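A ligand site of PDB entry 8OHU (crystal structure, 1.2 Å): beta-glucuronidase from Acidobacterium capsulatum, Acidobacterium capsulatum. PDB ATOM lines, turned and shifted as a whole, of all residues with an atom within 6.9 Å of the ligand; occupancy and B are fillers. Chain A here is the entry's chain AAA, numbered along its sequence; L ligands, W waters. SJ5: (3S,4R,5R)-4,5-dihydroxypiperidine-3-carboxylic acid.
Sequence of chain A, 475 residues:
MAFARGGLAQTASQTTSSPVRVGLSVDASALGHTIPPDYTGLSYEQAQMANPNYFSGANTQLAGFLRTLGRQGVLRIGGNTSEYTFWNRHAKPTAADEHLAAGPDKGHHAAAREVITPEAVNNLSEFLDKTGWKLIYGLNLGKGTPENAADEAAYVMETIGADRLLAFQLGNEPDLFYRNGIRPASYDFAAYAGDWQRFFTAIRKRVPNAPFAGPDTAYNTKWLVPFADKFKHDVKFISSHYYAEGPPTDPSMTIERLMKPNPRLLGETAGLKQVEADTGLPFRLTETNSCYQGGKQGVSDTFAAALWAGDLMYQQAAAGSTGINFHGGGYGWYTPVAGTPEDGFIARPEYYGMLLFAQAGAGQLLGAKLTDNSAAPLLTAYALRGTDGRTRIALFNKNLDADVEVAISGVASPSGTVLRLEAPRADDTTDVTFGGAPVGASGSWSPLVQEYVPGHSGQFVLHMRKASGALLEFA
The backbone NH (N) of Asp 105 sits at hydrogen-bond distance from an oxygen (O4) of the ligand, at 3.1 Å.
The backbone carbonyl oxygen of Asp 105 is in hydrogen-bond range of an oxygen (O4) of the ligand (2.8 Å).
The side-chain carboxylate of Glu 287 is in salt-bridge range of a nitrogen (N) of the ligand (2.6 Å).
N of the ligand is in salt-bridge range of OE2 of Glu 173, at 3.1 Å.
N of Asn 80 lies within hydrogen-bond range of O3 of the ligand (2.7 Å).
The side-chain carboxylate (OE2) of Glu 45 lies within hydrogen-bond range of an oxygen (O3) of the ligand, at 2.7 Å.
An oxygen (O62) of the ligand lies within hydrogen-bond range of the backbone NH of Gly 294, 2.9 Å away.
An oxygen (O61) of the ligand is in hydrogen-bond range of the backbone NH (N) of Gln 293, 2.7 Å away.
An oxygen (O62) of the ligand lies within hydrogen-bond range of the side-chain hydroxyl (OH) of Tyr 334, 2.6 Å away.
NH2 of Arg 76 sits at hydrogen-bond distance from OD1 of Asn 172.
OE2 of Glu 173 lies within hydrogen-bond range of ND1 of His 241 (2.7 Å).
The side-chain carboxylate (OE2) of Glu 45 sits at hydrogen-bond distance from a ring nitrogen (NE2) of His 327, at 2.9 Å.
The side-chain carboxylate (OE1) of Glu 45 lies within hydrogen-bond range of the side-chain hydroxyl (OG1) of Thr 81.
The side-chain carboxylate of Glu 287 lies within hydrogen-bond range of the side-chain hydroxyl of Tyr 243, 2.6 Å away.
OE1 of Glu 287 lies within salt-bridge range of NH1 of Arg 76, 2.8 Å away.
The side-chain amide nitrogen (ND2) of Asn 172 lies within hydrogen-bond range of the side-chain amide oxygen (OD1) of Asn 80, at 3.2 Å.
The side-chain carboxylate (OE2) of Glu 45 sits at hydrogen-bond distance from the backbone NH (N) of Asp 105 (2.9 Å).
Residues that only touch the ligand: Tyr 292 (3.5 Å), Gly 79 (3.5 Å), His 327 (3.5 Å), Tyr 243 (3.6 Å), Pro 104 (3.7 Å) and Asn 172 (3.97 Å).
The nearest printed residue that does not touch the ligand is Cys 291 (4.3 Å).
Water W1 lies within hydrogen-bond range of O61 of the ligand and ND2 of Asn 80.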
ATOM      1  N   GLU A  45      -3.757 -26.097 -12.587  1.00  0.00           N
ATOM      2  CA  GLU A  45      -4.005 -26.904 -13.799  1.00  0.00           C
ATOM      3  C   GLU A  45      -5.448 -26.778 -14.251  1.00  0.00           C
ATOM      4  O   GLU A  45      -6.389 -26.915 -13.499  1.00  0.00           O
ATOM      5  CB  GLU A  45      -3.715 -28.353 -13.467  1.00  0.00           C
ATOM      6  CG  GLU A  45      -2.238 -28.647 -13.220  1.00  0.00           C
ATOM      7  CD  GLU A  45      -1.315 -28.503 -14.400  1.00  0.00           C
ATOM      8  OE1 GLU A  45      -1.784 -28.528 -15.562  1.00  0.00           O
ATOM      9  OE2 GLU A  45      -0.087 -28.394 -14.161  1.00  0.00           O
ATOM     10  N   ARG A  76      -4.857 -17.816 -12.288  1.00  0.00           N
ATOM     11  CA  ARG A  76      -4.527 -18.319 -13.622  1.00  0.00           C
ATOM     12  C   ARG A  76      -4.805 -19.813 -13.681  1.00  0.00           C
ATOM     13  O   ARG A  76      -4.379 -20.548 -12.783  1.00  0.00           O
ATOM     14  CB  ARG A  76      -3.081 -17.978 -14.016  1.00  0.00           C
ATOM     15  CG  ARG A  76      -2.676 -18.517 -15.391  1.00  0.00           C
ATOM     16  CD  ARG A  76      -1.928 -19.826 -15.347  1.00  0.00           C
ATOM     17  NE  ARG A  76      -1.482 -20.327 -16.634  1.00  0.00           N
ATOM     18  CZ  ARG A  76      -0.541 -21.278 -16.769  1.00  0.00           C
ATOM     19  NH1 ARG A  76      -0.026 -21.816 -15.685  1.00  0.00           N
ATOM     20  NH2 ARG A  76      -0.224 -21.666 -17.969  1.00  0.00           N
ATOM     21  N   GLY A  78      -4.357 -23.043 -16.319  1.00  0.00           N
ATOM     22  CA  GLY A  78      -3.696 -23.438 -17.553  1.00  0.00           C
ATOM     23  C   GLY A  78      -2.802 -24.641 -17.331  1.00  0.00           C
ATOM     24  O   GLY A  78      -3.280 -25.708 -16.922  1.00  0.00           O
ATOM     25  N   GLY A  79      -1.493 -24.510 -17.598  1.00  0.00           N
ATOM     26  CA  GLY A  79      -0.570 -25.609 -17.376  1.00  0.00           C
ATOM     27  C   GLY A  79      -0.610 -26.658 -18.442  1.00  0.00           C
ATOM     28  O   GLY A  79      -1.337 -26.562 -19.426  1.00  0.00           O
ATOM     29  N   ASN A  80       0.166 -27.695 -18.240  1.00  0.00           N
ATOM     30  CA  ASN A  80       0.285 -28.777 -19.254  1.00  0.00           C
ATOM     31  C   ASN A  80      -1.076 -29.417 -19.482  1.00  0.00           C
ATOM     32  O   ASN A  80      -1.384 -29.874 -20.601  1.00  0.00           O
ATOM     33  CB  ASN A  80       1.245 -29.866 -18.746  1.00  0.00           C
ATOM     34  CG  ASN A  80       2.694 -29.483 -18.776  1.00  0.00           C
ATOM     35  OD1 ASN A  80       3.042 -28.458 -19.379  1.00  0.00           O
ATOM     36  ND2 ASN A  80       3.505 -30.258 -18.039  1.00  0.00           N
ATOM     37  N   THR A  81      -1.921 -29.481 -18.457  1.00  0.00           N
ATOM     38  CA  THR A  81      -3.218 -30.170 -18.604  1.00  0.00           C
ATOM     39  C   THR A  81      -4.125 -29.379 -19.531  1.00  0.00           C
ATOM     40  O   THR A  81      -5.139 -29.935 -19.985  1.00  0.00           O
ATOM     41  CB  THR A  81      -3.904 -30.483 -17.285  1.00  0.00           C
ATOM     42  OG1 THR A  81      -4.220 -29.258 -16.615  1.00  0.00           O
ATOM     43  CG2 THR A  81      -3.087 -31.422 -16.451  1.00  0.00           C
ATOM     44  N   SER A  82      -3.848 -28.113 -19.837  1.00  0.00           N
ATOM     45  CA  SER A  82      -4.698 -27.316 -20.768  1.00  0.00           C
ATOM     46  C   SER A  82      -4.668 -27.908 -22.163  1.00  0.00           C
ATOM     47  O   SER A  82      -5.639 -27.630 -22.893  1.00  0.00           O
ATOM     48  CB  SER A  82      -4.339 -25.893 -20.736  1.00  0.00           C
ATOM     49  OG  SER A  82      -3.123 -25.686 -21.322  1.00  0.00           O
ATOM     50  N   GLY A 103      -3.331 -32.004  -9.115  1.00  0.00           N
ATOM     51  CA  GLY A 103      -2.114 -31.312  -8.721  1.00  0.00           C
ATOM     52  C   GLY A 103      -1.309 -30.920  -9.941  1.00  0.00           C
ATOM     53  O   GLY A 103      -1.607 -31.297 -11.091  1.00  0.00           O
ATOM     54  N   PRO A 104      -0.218 -30.171  -9.725  1.00  0.00           N
ATOM     55  CA  PRO A 104       0.641 -29.787 -10.838  1.00  0.00           C
ATOM     56  C   PRO A 104       1.043 -30.983 -11.674  1.00  0.00           C
ATOM     57  O   PRO A 104       1.455 -32.027 -11.148  1.00  0.00           O
ATOM     58  CB  PRO A 104       1.843 -29.175 -10.115  1.00  0.00           C
ATOM     59  CG  PRO A 104       1.260 -28.624  -8.891  1.00  0.00           C
ATOM     60  CD  PRO A 104       0.216 -29.616  -8.434  1.00  0.00           C
ATOM     61  N   ASP A 105       1.026 -30.793 -12.990  1.00  0.00           N
ATOM     62  CA  ASP A 105       1.419 -31.882 -13.888  1.00  0.00           C
ATOM     63  C   ASP A 105       2.903 -32.139 -13.724  1.00  0.00           C
ATOM     64  O   ASP A 105       3.708 -31.216 -13.646  1.00  0.00           O
ATOM     65  CB  ASP A 105       1.055 -31.465 -15.302  1.00  0.00           C
ATOM     66  CG  ASP A 105       1.249 -32.626 -16.277  1.00  0.00           C
ATOM     67  OD1 ASP A 105       0.370 -33.525 -16.321  1.00  0.00           O
ATOM     68  OD2 ASP A 105       2.335 -32.663 -16.903  1.00  0.00           O
ATOM     69  N   LYS A 106       3.295 -33.421 -13.741  1.00  0.00           N
ATOM     70  CA  LYS A 106       4.738 -33.751 -13.508  1.00  0.00           C
ATOM     71  C   LYS A 106       5.524 -33.778 -14.813  1.00  0.00           C
ATOM     72  O   LYS A 106       6.781 -33.854 -14.729  1.00  0.00           O
ATOM     73  CB  LYS A 106       4.837 -35.014 -12.650  1.00  0.00           C
ATOM     74  CG  LYS A 106       4.147 -34.886 -11.306  1.00  0.00           C
ATOM     75  CD  LYS A 106       4.231 -36.173 -10.441  1.00  0.00           C
ATOM     76  CE  LYS A 106       3.753 -35.973  -9.019  1.00  0.00           C
ATOM     77  NZ  LYS A 106       2.288 -35.995  -8.909  1.00  0.00           N
ATOM     78  N   GLY A 107       4.877 -33.700 -15.983  1.00  0.00           N
ATOM     79  CA  GLY A 107       5.528 -33.468 -17.298  1.00  0.00           C
ATOM     80  C   GLY A 107       6.305 -34.675 -17.808  1.00  0.00           C
ATOM     81  O   GLY A 107       7.191 -34.479 -18.669  1.00  0.00           O
ATOM     82  N   ASN A 172      -0.348 -23.414 -23.390  1.00  0.00           N
ATOM     83  CA  ASN A 172       0.683 -23.328 -22.319  1.00  0.00           C
ATOM     84  C   ASN A 172       2.014 -23.778 -22.871  1.00  0.00           C
ATOM     85  O   ASN A 172       2.079 -24.873 -23.454  1.00  0.00           O
ATOM     86  CB  ASN A 172       0.250 -24.212 -21.174  1.00  0.00           C
ATOM     87  CG  ASN A 172       1.359 -24.439 -20.159  1.00  0.00           C
ATOM     88  OD1 ASN A 172       1.578 -23.621 -19.253  1.00  0.00           O
ATOM     89  ND2 ASN A 172       1.983 -25.596 -20.242  1.00  0.00           N
ATOM     90  N   GLU A 173       3.059 -22.995 -22.697  1.00  0.00           N
ATOM     91  CA  GLU A 173       4.441 -23.427 -23.040  1.00  0.00           C
ATOM     92  C   GLU A 173       4.472 -24.089 -24.433  1.00  0.00           C
ATOM     93  O   GLU A 173       4.925 -25.232 -24.593  1.00  0.00           O
ATOM     94  CB  GLU A 173       5.011 -24.376 -21.983  1.00  0.00           C
ATOM     95  CG  GLU A 173       5.161 -23.668 -20.628  1.00  0.00           C
ATOM     96  CD  GLU A 173       5.536 -24.462 -19.401  1.00  0.00           C
ATOM     97  OE1 GLU A 173       5.392 -25.674 -19.383  1.00  0.00           O
ATOM     98  OE2 GLU A 173       5.915 -23.869 -18.366  1.00  0.00           O
ATOM     99  N   LEU A 176       7.416 -26.066 -25.777  1.00  0.00           N
ATOM    100  CA  LEU A 176       7.651 -27.427 -25.236  1.00  0.00           C
ATOM    101  C   LEU A 176       6.584 -28.394 -25.713  1.00  0.00           C
ATOM    102  O   LEU A 176       6.543 -29.548 -25.191  1.00  0.00           O
ATOM    103  CB  LEU A 176       7.662 -27.442 -23.720  1.00  0.00           C
ATOM    104  CG  LEU A 176       8.629 -26.447 -23.089  1.00  0.00           C
ATOM    105  CD1 LEU A 176       8.541 -26.491 -21.566  1.00  0.00           C
ATOM    106  CD2 LEU A 176      10.063 -26.657 -23.534  1.00  0.00           C
ATOM    107  N   HIS A 241       6.827 -17.525 -17.905  1.00  0.00           N
ATOM    108  CA  HIS A 241       6.996 -18.520 -16.817  1.00  0.00           C
ATOM    109  C   HIS A 241       8.399 -18.444 -16.237  1.00  0.00           C
ATOM    110  O   HIS A 241       9.347 -18.022 -16.933  1.00  0.00           O
ATOM    111  CB  HIS A 241       6.721 -19.947 -17.300  1.00  0.00           C
ATOM    112  CG  HIS A 241       5.290 -20.150 -17.714  1.00  0.00           C
ATOM    113  ND1 HIS A 241       4.834 -21.410 -18.018  1.00  0.00           N
ATOM    114  CD2 HIS A 241       4.231 -19.313 -17.832  1.00  0.00           C
ATOM    115  CE1 HIS A 241       3.536 -21.303 -18.350  1.00  0.00           C
ATOM    116  NE2 HIS A 241       3.141 -20.068 -18.220  1.00  0.00           N
ATOM    117  N   TYR A 243      10.898 -21.005 -13.503  1.00  0.00           N
ATOM    118  CA  TYR A 243      11.247 -21.972 -12.452  1.00  0.00           C
ATOM    119  C   TYR A 243      12.696 -21.730 -12.070  1.00  0.00           C
ATOM    120  O   TYR A 243      13.558 -21.593 -12.973  1.00  0.00           O
ATOM    121  CB  TYR A 243      10.977 -23.410 -12.905  1.00  0.00           C
ATOM    122  CG  TYR A 243       9.512 -23.735 -12.863  1.00  0.00           C
ATOM    123  CD1 TYR A 243       8.655 -23.287 -13.855  1.00  0.00           C
ATOM    124  CD2 TYR A 243       8.941 -24.350 -11.782  1.00  0.00           C
ATOM    125  CE1 TYR A 243       7.254 -23.453 -13.739  1.00  0.00           C
ATOM    126  CE2 TYR A 243       7.581 -24.545 -11.644  1.00  0.00           C
ATOM    127  CZ  TYR A 243       6.731 -24.090 -12.632  1.00  0.00           C
ATOM    128  OH  TYR A 243       5.385 -24.236 -12.425  1.00  0.00           O
ATOM    129  N   GLU A 287       3.168 -18.115 -14.484  1.00  0.00           N
ATOM    130  CA  GLU A 287       3.383 -19.451 -13.880  1.00  0.00           C
ATOM    131  C   GLU A 287       4.791 -19.527 -13.351  1.00  0.00           C
ATOM    132  O   GLU A 287       5.747 -19.362 -14.119  1.00  0.00           O
ATOM    133  CB  GLU A 287       3.096 -20.622 -14.796  1.00  0.00           C
ATOM    134  CG  GLU A 287       2.949 -21.918 -14.041  1.00  0.00           C
ATOM    135  CD  GLU A 287       3.091 -23.116 -14.913  1.00  0.00           C
ATOM    136  OE1 GLU A 287       2.309 -23.352 -15.821  1.00  0.00           O
ATOM    137  OE2 GLU A 287       4.106 -23.858 -14.700  1.00  0.00           O
ATOM    138  N   ASN A 289       7.306 -21.496 -10.046  1.00  0.00           N
ATOM    139  CA  ASN A 289       7.595 -22.084  -8.740  1.00  0.00           C
ATOM    140  C   ASN A 289       9.049 -22.484  -8.696  1.00  0.00           C
ATOM    141  O   ASN A 289       9.845 -22.167  -9.582  1.00  0.00           O
ATOM    142  CB  ASN A 289       6.567 -23.171  -8.380  1.00  0.00           C
ATOM    143  CG  ASN A 289       6.145 -22.941  -6.946  1.00  0.00           C
ATOM    144  OD1 ASN A 289       7.009 -22.735  -6.075  1.00  0.00           O
ATOM    145  ND2 ASN A 289       4.851 -22.915  -6.622  1.00  0.00           N
ATOM    146  N   CYS A 291      10.861 -25.525  -8.378  1.00  0.00           N
ATOM    147  CA  CYS A 291      11.402 -26.705  -9.107  1.00  0.00           C
ATOM    148  C   CYS A 291      10.309 -27.231 -10.017  1.00  0.00           C
ATOM    149  O   CYS A 291       9.144 -27.236  -9.618  1.00  0.00           O
ATOM    150  CB  CYS A 291      11.897 -27.803  -8.166  1.00  0.00           C
ATOM    151  SG  CYS A 291      13.152 -27.233  -6.998  1.00  0.00           S
ATOM    152  N   TYR A 292      10.647 -27.678 -11.217  1.00  0.00           N
ATOM    153  CA  TYR A 292       9.622 -28.124 -12.176  1.00  0.00           C
ATOM    154  C   TYR A 292       9.371 -29.594 -11.905  1.00  0.00           C
ATOM    155  O   TYR A 292       9.717 -30.162 -10.844  1.00  0.00           O
ATOM    156  CB  TYR A 292       9.863 -27.580 -13.609  1.00  0.00           C
ATOM    157  CG  TYR A 292      11.176 -27.922 -14.212  1.00  0.00           C
ATOM    158  CD1 TYR A 292      11.434 -29.193 -14.714  1.00  0.00           C
ATOM    159  CD2 TYR A 292      12.209 -27.014 -14.232  1.00  0.00           C
ATOM    160  CE1 TYR A 292      12.669 -29.539 -15.241  1.00  0.00           C
ATOM    161  CE2 TYR A 292      13.457 -27.335 -14.743  1.00  0.00           C
ATOM    162  CZ  TYR A 292      13.695 -28.613 -15.251  1.00  0.00           C
ATOM    163  OH  TYR A 292      14.932 -28.933 -15.726  1.00  0.00           O
ATOM    164  N   GLN A 293       8.559 -30.187 -12.786  1.00  0.00           N
ATOM    165  CA  GLN A 293       8.085 -31.576 -12.649  1.00  0.00           C
ATOM    166  C   GLN A 293       7.316 -31.756 -11.359  1.00  0.00           C
ATOM    167  O   GLN A 293       7.381 -32.867 -10.764  1.00  0.00           O
ATOM    168  CB  GLN A 293       9.267 -32.551 -12.864  1.00  0.00           C
ATOM    169  CG  GLN A 293       9.955 -32.315 -14.196  1.00  0.00           C
ATOM    170  CD  GLN A 293      10.548 -33.571 -14.791  1.00  0.00           C
ATOM    171  OE1 GLN A 293      11.503 -34.122 -14.253  1.00  0.00           O
ATOM    172  NE2 GLN A 293       9.930 -34.038 -15.860  1.00  0.00           N
ATOM    173  N   GLY A 294       6.544 -30.759 -10.890  1.00  0.00           N
ATOM    174  CA  GLY A 294       5.718 -30.672  -9.693  1.00  0.00           C
ATOM    175  C   GLY A 294       6.486 -30.450  -8.388  1.00  0.00           C
ATOM    176  O   GLY A 294       5.836 -30.385  -7.333  1.00  0.00           O
ATOM    177  N   GLY A 295       7.772 -30.111  -8.496  1.00  0.00           N
ATOM    178  CA  GLY A 295       8.536 -29.709  -7.313  1.00  0.00           C
ATOM    179  C   GLY A 295       9.421 -30.828  -6.832  1.00  0.00           C
ATOM    180  O   GLY A 295       9.229 -31.975  -7.231  1.00  0.00           O
ATOM    181  N   HIS A 327       2.396 -21.568  -9.214  1.00  0.00           N
ATOM    182  CA  HIS A 327       1.695 -22.786  -9.633  1.00  0.00           C
ATOM    183  C   HIS A 327       1.520 -23.714  -8.435  1.00  0.00           C
ATOM    184  O   HIS A 327       2.262 -23.719  -7.460  1.00  0.00           O
ATOM    185  CB  HIS A 327       2.446 -23.466 -10.759  1.00  0.00           C
ATOM    186  CG  HIS A 327       1.616 -24.398 -11.564  1.00  0.00           C
ATOM    187  ND1 HIS A 327       0.446 -23.982 -12.161  1.00  0.00           N
ATOM    188  CD2 HIS A 327       1.779 -25.703 -11.880  1.00  0.00           C
ATOM    189  CE1 HIS A 327      -0.065 -25.006 -12.807  1.00  0.00           C
ATOM    190  NE2 HIS A 327       0.724 -26.091 -12.672  1.00  0.00           N
ATOM    191  N   TYR A 334       5.307 -28.117  -4.459  1.00  0.00           N
ATOM    192  CA  TYR A 334       5.485 -26.653  -4.393  1.00  0.00           C
ATOM    193  C   TYR A 334       4.178 -25.880  -4.190  1.00  0.00           C
ATOM    194  O   TYR A 334       4.229 -24.650  -4.205  1.00  0.00           O
ATOM    195  CB  TYR A 334       6.246 -26.082  -5.607  1.00  0.00           C
ATOM    196  CG  TYR A 334       5.720 -26.364  -6.990  1.00  0.00           C
ATOM    197  CD1 TYR A 334       4.402 -26.108  -7.357  1.00  0.00           C
ATOM    198  CD2 TYR A 334       6.563 -26.876  -7.962  1.00  0.00           C
ATOM    199  CE1 TYR A 334       3.959 -26.380  -8.631  1.00  0.00           C
ATOM    200  CE2 TYR A 334       6.127 -27.137  -9.240  1.00  0.00           C
ATOM    201  CZ  TYR A 334       4.806 -26.908  -9.565  1.00  0.00           C
ATOM    202  OH  TYR A 334       4.331 -27.185 -10.808  1.00  0.00           O
HETATM  203  C2  SJ5 L   1       3.564 -26.484 -16.715  1.00  0.00           C
HETATM  204  C3  SJ5 L   1       2.855 -27.096 -15.523  1.00  0.00           C
HETATM  205  O3  SJ5 L   1       1.745 -27.831 -15.996  1.00  0.00           O
HETATM  206  N   SJ5 L   1       4.757 -25.791 -16.287  1.00  0.00           N
HETATM  207  C7  SJ5 L   1       5.707 -26.648 -15.604  1.00  0.00           C
HETATM  208  C5  SJ5 L   1       5.080 -27.270 -14.363  1.00  0.00           C
HETATM  209  C6  SJ5 L   1       6.052 -28.219 -13.679  1.00  0.00           C
HETATM  210  O62 SJ5 L   1       6.103 -28.296 -12.429  1.00  0.00           O
HETATM  211  C4  SJ5 L   1       3.799 -28.008 -14.757  1.00  0.00           C
HETATM  212  O4  SJ5 L   1       3.106 -28.505 -13.584  1.00  0.00           O
HETATM  213  O61 SJ5 L   1       6.790 -28.926 -14.415  1.00  0.00           O
HETATM  214  O   HOH W   1       6.404 -29.874 -17.149  1.00  0.00           O
